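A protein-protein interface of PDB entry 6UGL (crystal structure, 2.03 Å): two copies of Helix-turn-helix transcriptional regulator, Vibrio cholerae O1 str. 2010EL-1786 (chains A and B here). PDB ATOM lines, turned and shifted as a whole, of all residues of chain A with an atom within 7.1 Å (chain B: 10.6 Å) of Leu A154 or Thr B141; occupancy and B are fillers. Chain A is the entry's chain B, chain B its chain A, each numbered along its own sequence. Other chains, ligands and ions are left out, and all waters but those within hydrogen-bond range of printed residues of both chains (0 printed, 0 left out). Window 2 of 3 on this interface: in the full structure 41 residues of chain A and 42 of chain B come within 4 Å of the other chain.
The backbone carbonyl oxygen (O) of Leu B139 is in hydrogen-bond range of the side-chain amino group (NZ) of Lys A155 (3.4 Å). The backbone carbonyl oxygen (O) of Thr B137 lies within hydrogen-bond range of the side-chain amino group (NZ) of Lys A155 (2.5 Å). The backbone NH of Thr B141 sits at hydrogen-bond distance from the backbone carbonyl oxygen of Leu A154. The backbone NH (N) of Leu A156 is in hydrogen-bond range of the backbone carbonyl oxygen (O) of Leu B139 (3.3 Å). The indole nitrogen of Trp B132 is in hydrogen-bond range of the backbone carbonyl oxygen of Arg A213.
O of Lys A155 is in hydrogen-bond range of NZ of Lys A197 (2.7 Å). The side-chain hydroxyl (OG1) of Thr B141 lies within hydrogen-bond range of the backbone carbonyl oxygen (O) of His B131, at 3.0 Å. O of Val B133 sits at hydrogen-bond distance from N of Ser B140, 2.8 Å away.
Ser B140 touches Leu A154 (CA to O, 3.2 Å). Arg B135 touches Lys A155. NZ of Lys A155 touches C of Gly B138, 3.9 Å away. CD1 of Leu A156 touches CH2 of Trp B132, 3.7 Å away. Leu A156 touches Thr B137 (O to O, 3.9 Å). Leu A156 touches Gly B138 (O to CA, 3.5 Å). Phe A198 touches Trp B132 (CZ to CZ2, 3.9 Å).
Of chain B, only Ser B140 and Thr B141 come within 4 Å of Leu A154. Of chain A, only Leu A154 comes within 4 Å of Thr B141. No residue of chain B comes within 4 Å of Thr A153. No residue of chain B comes within 4 Å of Lys A197. Of chain B, only Trp B132 comes within 4 Å of Phe A198. Of the printed residues of chain B, Arg A213 touches Trp B132. Of the printed residues of chain A, Trp B132 touches Leu A156 (3.7 Å), Phe A198 (3.9 Å) and Arg A213 (3.0 Å). Of the printed residues of chain A, Arg B135 touches Lys A155.
Of the 13 printed residues of chain B, 7 touch a printed residue of chain A. Hydrophobic or aromatic side chains of chain B within 4 Å of the printed part of chain A: Trp B132. Along chain A the printed residues that touch a printed residue of chain B span positions 154 to 213. Among the printed residues, 12 pairs touch across the chains. Among the printed residues, no Asp or Glu carboxylate lies within 4 Å of a Lys or Arg side-chain nitrogen of the other chain.
Position printed for both chains: 213. Of the 12 pairs that touch across the chains among the printed residues, none has its exchanged pair printed and touching as well.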
ATOM      1  N   THR A 153      14.501  -9.485  -7.941  1.00  0.00           N
ATOM      2  CA  THR A 153      13.080  -9.789  -7.756  1.00  0.00           C
ATOM      3  C   THR A 153      12.195  -8.590  -8.076  1.00  0.00           C
ATOM      4  O   THR A 153      12.294  -7.554  -7.420  1.00  0.00           O
ATOM      5  CB  THR A 153      12.824 -10.258  -6.330  1.00  0.00           C
ATOM      6  N   LEU A 154      11.330  -8.727  -9.080  1.00  0.00           N
ATOM      7  CA  LEU A 154      10.341  -7.701  -9.411  1.00  0.00           C
ATOM      8  C   LEU A 154       9.054  -7.988  -8.644  1.00  0.00           C
ATOM      9  O   LEU A 154       8.367  -8.977  -8.917  1.00  0.00           O
ATOM     10  CB  LEU A 154      10.075  -7.660 -10.914  1.00  0.00           C
ATOM     11  CG  LEU A 154       8.891  -6.782 -11.326  1.00  0.00           C
ATOM     12  CD1 LEU A 154       9.154  -5.333 -10.974  1.00  0.00           C
ATOM     13  CD2 LEU A 154       8.576  -6.924 -12.804  1.00  0.00           C
ATOM     14  N   LYS A 155       8.715  -7.115  -7.699  1.00  0.00           N
ATOM     15  CA  LYS A 155       7.586  -7.319  -6.802  1.00  0.00           C
ATOM     16  C   LYS A 155       6.504  -6.274  -7.054  1.00  0.00           C
ATOM     17  O   LYS A 155       6.796  -5.080  -7.179  1.00  0.00           O
ATOM     18  CB  LYS A 155       8.040  -7.252  -5.341  1.00  0.00           C
ATOM     19  CG  LYS A 155       6.928  -7.465  -4.332  1.00  0.00           C
ATOM     20  CD  LYS A 155       6.595  -8.937  -4.195  1.00  0.00           C
ATOM     21  CE  LYS A 155       5.549  -9.172  -3.119  1.00  0.00           C
ATOM     22  NZ  LYS A 155       4.187  -9.239  -3.689  1.00  0.00           N
ATOM     23  N   LEU A 156       5.250  -6.725  -7.121  1.00  0.00           N
ATOM     24  CA  LEU A 156       4.106  -5.848  -7.325  1.00  0.00           C
ATOM     25  C   LEU A 156       3.154  -5.959  -6.142  1.00  0.00           C
ATOM     26  O   LEU A 156       2.849  -7.064  -5.682  1.00  0.00           O
ATOM     27  CB  LEU A 156       3.364  -6.190  -8.625  1.00  0.00           C
ATOM     28  CG  LEU A 156       4.189  -6.252  -9.918  1.00  0.00           C
ATOM     29  CD1 LEU A 156       3.264  -6.412 -11.123  1.00  0.00           C
ATOM     30  CD2 LEU A 156       5.089  -5.042 -10.090  1.00  0.00           C
ATOM     31  N   LYS A 193       4.722   4.049 -10.435  1.00  0.00           N
ATOM     32  CA  LYS A 193       5.430   3.035  -9.655  1.00  0.00           C
ATOM     33  C   LYS A 193       5.686   1.781 -10.481  1.00  0.00           C
ATOM     34  O   LYS A 193       6.743   1.150 -10.352  1.00  0.00           O
ATOM     35  CB  LYS A 193       4.636   2.690  -8.396  1.00  0.00           C
ATOM     36  CG  LYS A 193       4.558   3.824  -7.383  1.00  0.00           C
ATOM     37  CD  LYS A 193       3.664   3.472  -6.202  1.00  0.00           C
ATOM     38  CE  LYS A 193       3.599   4.623  -5.207  1.00  0.00           C
ATOM     39  NZ  LYS A 193       2.621   4.365  -4.112  1.00  0.00           N
ATOM     40  N   LEU A 194       4.733   1.406 -11.342  1.00  0.00           N
ATOM     41  CA  LEU A 194       4.925   0.261 -12.229  1.00  0.00           C
ATOM     42  C   LEU A 194       5.883   0.572 -13.372  1.00  0.00           C
ATOM     43  O   LEU A 194       6.622  -0.315 -13.812  1.00  0.00           O
ATOM     44  CB  LEU A 194       3.583  -0.200 -12.808  1.00  0.00           C
ATOM     45  CG  LEU A 194       2.578  -0.904 -11.898  1.00  0.00           C
ATOM     46  CD1 LEU A 194       1.223  -0.924 -12.579  1.00  0.00           C
ATOM     47  CD2 LEU A 194       3.031  -2.317 -11.570  1.00  0.00           C
ATOM     48  N   SER A 196       8.508   2.507 -13.306  1.00  0.00           N
ATOM     49  CA  SER A 196       9.885   2.423 -12.831  1.00  0.00           C
ATOM     50  C   SER A 196      10.245   1.011 -12.383  1.00  0.00           C
ATOM     51  O   SER A 196      11.394   0.592 -12.553  1.00  0.00           O
ATOM     52  CB  SER A 196      10.126   3.423 -11.694  1.00  0.00           C
ATOM     53  OG  SER A 196       9.682   2.918 -10.446  1.00  0.00           O
ATOM     54  N   LYS A 197       9.289   0.259 -11.829  1.00  0.00           N
ATOM     55  CA  LYS A 197       9.589  -1.105 -11.400  1.00  0.00           C
ATOM     56  C   LYS A 197       9.916  -2.000 -12.587  1.00  0.00           C
ATOM     57  O   LYS A 197      10.816  -2.843 -12.503  1.00  0.00           O
ATOM     58  CB  LYS A 197       8.427  -1.688 -10.600  1.00  0.00           C
ATOM     59  CG  LYS A 197       8.455  -1.326  -9.126  1.00  0.00           C
ATOM     60  CD  LYS A 197       7.381  -2.091  -8.370  1.00  0.00           C
ATOM     61  CE  LYS A 197       7.362  -1.692  -6.905  1.00  0.00           C
ATOM     62  NZ  LYS A 197       6.451  -2.567  -6.130  1.00  0.00           N
ATOM     63  N   PHE A 198       9.202  -1.835 -13.700  1.00  0.00           N
ATOM     64  CA  PHE A 198       9.499  -2.584 -14.917  1.00  0.00           C
ATOM     65  C   PHE A 198      10.621  -1.956 -15.737  1.00  0.00           C
ATOM     66  O   PHE A 198      11.085  -2.578 -16.698  1.00  0.00           O
ATOM     67  CB  PHE A 198       8.243  -2.708 -15.798  1.00  0.00           C
ATOM     68  CG  PHE A 198       7.359  -3.878 -15.453  1.00  0.00           C
ATOM     69  CD1 PHE A 198       6.401  -3.772 -14.458  1.00  0.00           C
ATOM     70  CD2 PHE A 198       7.468  -5.074 -16.143  1.00  0.00           C
ATOM     71  CE1 PHE A 198       5.577  -4.847 -14.148  1.00  0.00           C
ATOM     72  CE2 PHE A 198       6.650  -6.152 -15.839  1.00  0.00           C
ATOM     73  CZ  PHE A 198       5.705  -6.040 -14.842  1.00  0.00           C
ATOM     74  N   GLY A 199      11.062  -0.750 -15.385  1.00  0.00           N
ATOM     75  CA  GLY A 199      12.051  -0.050 -16.174  1.00  0.00           C
ATOM     76  C   GLY A 199      11.533   0.544 -17.463  1.00  0.00           C
ATOM     77  O   GLY A 199      12.338   0.999 -18.284  1.00  0.00           O
ATOM     78  N   ARG A 213       6.616 -10.573 -20.233  1.00  0.00           N
ATOM     79  CA  ARG A 213       6.925 -11.398 -19.073  1.00  0.00           C
ATOM     80  C   ARG A 213       5.775 -12.314 -18.672  1.00  0.00           C
ATOM     81  O   ARG A 213       5.856 -12.973 -17.628  1.00  0.00           O
ATOM     82  CB  ARG A 213       7.318 -10.514 -17.892  1.00  0.00           C
ATOM     83  CG  ARG A 213       8.508  -9.648 -18.185  1.00  0.00           C
ATOM     84  CD  ARG A 213       9.051  -9.003 -16.936  1.00  0.00           C
ATOM     85  NE  ARG A 213      10.489  -8.798 -17.047  1.00  0.00           N
ATOM     86  CZ  ARG A 213      11.186  -7.951 -16.297  1.00  0.00           C
ATOM     87  NH1 ARG A 213      12.495  -7.834 -16.471  1.00  0.00           N
ATOM     88  NH2 ARG A 213      10.572  -7.215 -15.381  1.00  0.00           N
ATOM     89  N   HIS B 131       6.254 -17.243 -15.983  1.00  0.00           N
ATOM     90  CA  HIS B 131       7.181 -17.406 -14.866  1.00  0.00           C
ATOM     91  C   HIS B 131       6.875 -16.418 -13.739  1.00  0.00           C
ATOM     92  O   HIS B 131       7.784 -15.899 -13.085  1.00  0.00           O
ATOM     93  CB  HIS B 131       8.627 -17.239 -15.342  1.00  0.00           C
ATOM     94  N   TRP B 132       5.587 -16.157 -13.522  1.00  0.00           N
ATOM     95  CA  TRP B 132       5.133 -15.332 -12.410  1.00  0.00           C
ATOM     96  C   TRP B 132       4.795 -16.210 -11.208  1.00  0.00           C
ATOM     97  O   TRP B 132       4.340 -17.350 -11.353  1.00  0.00           O
ATOM     98  CB  TRP B 132       3.907 -14.503 -12.800  1.00  0.00           C
ATOM     99  CG  TRP B 132       4.198 -13.246 -13.569  1.00  0.00           C
ATOM    100  CD1 TRP B 132       4.222 -13.101 -14.928  1.00  0.00           C
ATOM    101  CD2 TRP B 132       4.484 -11.950 -13.023  1.00  0.00           C
ATOM    102  NE1 TRP B 132       4.515 -11.797 -15.259  1.00  0.00           N
ATOM    103  CE2 TRP B 132       4.679 -11.070 -14.110  1.00  0.00           C
ATOM    104  CE3 TRP B 132       4.597 -11.451 -11.723  1.00  0.00           C
ATOM    105  CZ2 TRP B 132       4.980  -9.719 -13.936  1.00  0.00           C
ATOM    106  CZ3 TRP B 132       4.900 -10.104 -11.548  1.00  0.00           C
ATOM    107  CH2 TRP B 132       5.088  -9.256 -12.650  1.00  0.00           C
ATOM    108  N   VAL B 133       5.012 -15.658 -10.017  1.00  0.00           N
ATOM    109  CA  VAL B 133       4.865 -16.380  -8.759  1.00  0.00           C
ATOM    110  C   VAL B 133       3.924 -15.594  -7.854  1.00  0.00           C
ATOM    111  O   VAL B 133       3.991 -14.361  -7.803  1.00  0.00           O
ATOM    112  CB  VAL B 133       6.233 -16.588  -8.069  1.00  0.00           C
ATOM    113  CG1 VAL B 133       6.104 -17.547  -6.896  1.00  0.00           C
ATOM    114  CG2 VAL B 133       7.275 -17.079  -9.068  1.00  0.00           C
ATOM    115  N   CYS B 134       3.049 -16.305  -7.139  1.00  0.00           N
ATOM    116  CA  CYS B 134       2.151 -15.669  -6.180  1.00  0.00           C
ATOM    117  C   CYS B 134       2.877 -15.431  -4.862  1.00  0.00           C
ATOM    118  O   CYS B 134       3.503 -16.346  -4.319  1.00  0.00           O
ATOM    119  CB  CYS B 134       0.911 -16.530  -5.921  1.00  0.00           C
ATOM    120  SG  CYS B 134      -0.086 -16.989  -7.359  1.00  0.00           S
ATOM    121  N   ARG B 135       2.777 -14.206  -4.342  1.00  0.00           N
ATOM    122  CA  ARG B 135       3.313 -13.818  -3.043  1.00  0.00           C
ATOM    123  C   ARG B 135       2.165 -13.590  -2.060  1.00  0.00           C
ATOM    124  O   ARG B 135       0.986 -13.699  -2.413  1.00  0.00           O
ATOM    125  CB  ARG B 135       4.187 -12.568  -3.172  1.00  0.00           C
ATOM    126  N   THR B 137       0.815 -10.880  -0.541  1.00  0.00           N
ATOM    127  CA  THR B 137      -0.021  -9.981  -1.322  1.00  0.00           C
ATOM    128  C   THR B 137       0.691  -9.699  -2.638  1.00  0.00           C
ATOM    129  O   THR B 137       1.881  -9.372  -2.641  1.00  0.00           O
ATOM    130  CB  THR B 137      -0.307  -8.672  -0.580  1.00  0.00           C
ATOM    131  OG1 THR B 137       0.898  -7.902  -0.465  1.00  0.00           O
ATOM    132  CG2 THR B 137      -0.857  -8.957   0.812  1.00  0.00           C
ATOM    133  N   GLY B 138      -0.025  -9.845  -3.745  1.00  0.00           N
ATOM    134  CA  GLY B 138       0.545  -9.562  -5.047  1.00  0.00           C
ATOM    135  C   GLY B 138       1.233 -10.765  -5.662  1.00  0.00           C
ATOM    136  O   GLY B 138       1.048 -11.913  -5.246  1.00  0.00           O
ATOM    137  N   LEU B 139       2.035 -10.486  -6.691  1.00  0.00           N
ATOM    138  CA  LEU B 139       2.836 -11.484  -7.397  1.00  0.00           C
ATOM    139  C   LEU B 139       4.286 -11.010  -7.447  1.00  0.00           C
ATOM    140  O   LEU B 139       4.614  -9.917  -6.976  1.00  0.00           O
ATOM    141  CB  LEU B 139       2.299 -11.744  -8.811  1.00  0.00           C
ATOM    142  CG  LEU B 139       1.039 -12.601  -8.973  1.00  0.00           C
ATOM    143  CD1 LEU B 139      -0.221 -11.822  -8.628  1.00  0.00           C
ATOM    144  CD2 LEU B 139       0.954 -13.165 -10.386  1.00  0.00           C
ATOM    145  N   SER B 140       5.165 -11.831  -8.025  1.00  0.00           N
ATOM    146  CA  SER B 140       6.575 -11.472  -8.090  1.00  0.00           C
ATOM    147  C   SER B 140       7.213 -12.027  -9.358  1.00  0.00           C
ATOM    148  O   SER B 140       6.738 -13.004  -9.950  1.00  0.00           O
ATOM    149  CB  SER B 140       7.344 -11.961  -6.851  1.00  0.00           C
ATOM    150  OG  SER B 140       7.364 -13.378  -6.775  1.00  0.00           O
ATOM    151  N   THR B 141       8.312 -11.379  -9.752  1.00  0.00           N
ATOM    152  CA  THR B 141       9.140 -11.736 -10.910  1.00  0.00           C
ATOM    153  C   THR B 141       8.359 -11.723 -12.216  1.00  0.00           C
ATOM    154  O   THR B 141       8.840 -11.198 -13.219  1.00  0.00           O
ATOM    155  CB  THR B 141       9.804 -13.126 -10.747  1.00  0.00           C
ATOM    156  OG1 THR B 141       8.819 -14.159 -10.884  1.00  0.00           O
ATOM    157  CG2 THR B 141      10.489 -13.237  -9.387  1.00  0.00           C
ATOM    158  N   ASP B 212       1.084 -21.892  -7.871  1.00  0.00           N
ATOM    159  CA  ASP B 212       1.544 -20.524  -7.666  1.00  0.00           C
ATOM    160  C   ASP B 212       2.376 -20.001  -8.827  1.00  0.00           C
ATOM    161  O   ASP B 212       2.699 -18.805  -8.844  1.00  0.00           O
ATOM    162  CB  ASP B 212       2.352 -20.430  -6.369  1.00  0.00           C
ATOM    163  CG  ASP B 212       1.486 -20.582  -5.129  1.00  0.00           C
ATOM    164  OD1 ASP B 212       0.250 -20.640  -5.283  1.00  0.00           O
ATOM    165  OD2 ASP B 212       2.037 -20.648  -4.008  1.00  0.00           O
ATOM    166  N   ARG B 213       2.726 -20.855  -9.788  1.00  0.00           N
ATOM    167  CA  ARG B 213       3.529 -20.476 -10.943  1.00  0.00           C
ATOM    168  C   ARG B 213       2.761 -20.590 -12.253  1.00  0.00           C
ATOM    169  O   ARG B 213       3.376 -20.561 -13.324  1.00  0.00           O
ATOM    170  CB  ARG B 213       4.807 -21.322 -10.996  1.00  0.00           C
ATOM    171  CG  ARG B 213       5.947 -20.686 -10.224  1.00  0.00           C
ATOM    172  CD  ARG B 213       7.057 -21.669  -9.876  1.00  0.00           C
ATOM    173  NE  ARG B 213       8.002 -21.073  -8.933  1.00  0.00           N
ATOM    174  CZ  ARG B 213       7.755 -20.891  -7.637  1.00  0.00           C
ATOM    175  NH1 ARG B 213       6.588 -21.267  -7.120  1.00  0.00           N
ATOM    176  NH2 ARG B 213       8.675 -20.333  -6.857  1.00  0.00           N
ATOM    177  N   GLY B 214       1.440 -20.722 -12.197  1.00  0.00           N
ATOM    178  CA  GLY B 214       0.629 -20.724 -13.395  1.00  0.00           C
ATOM    179  C   GLY B 214       0.527 -22.047 -14.113  1.00  0.00           C
ATOM    180  O   GLY B 214      -0.012 -22.087 -15.229  1.00  0.00           O
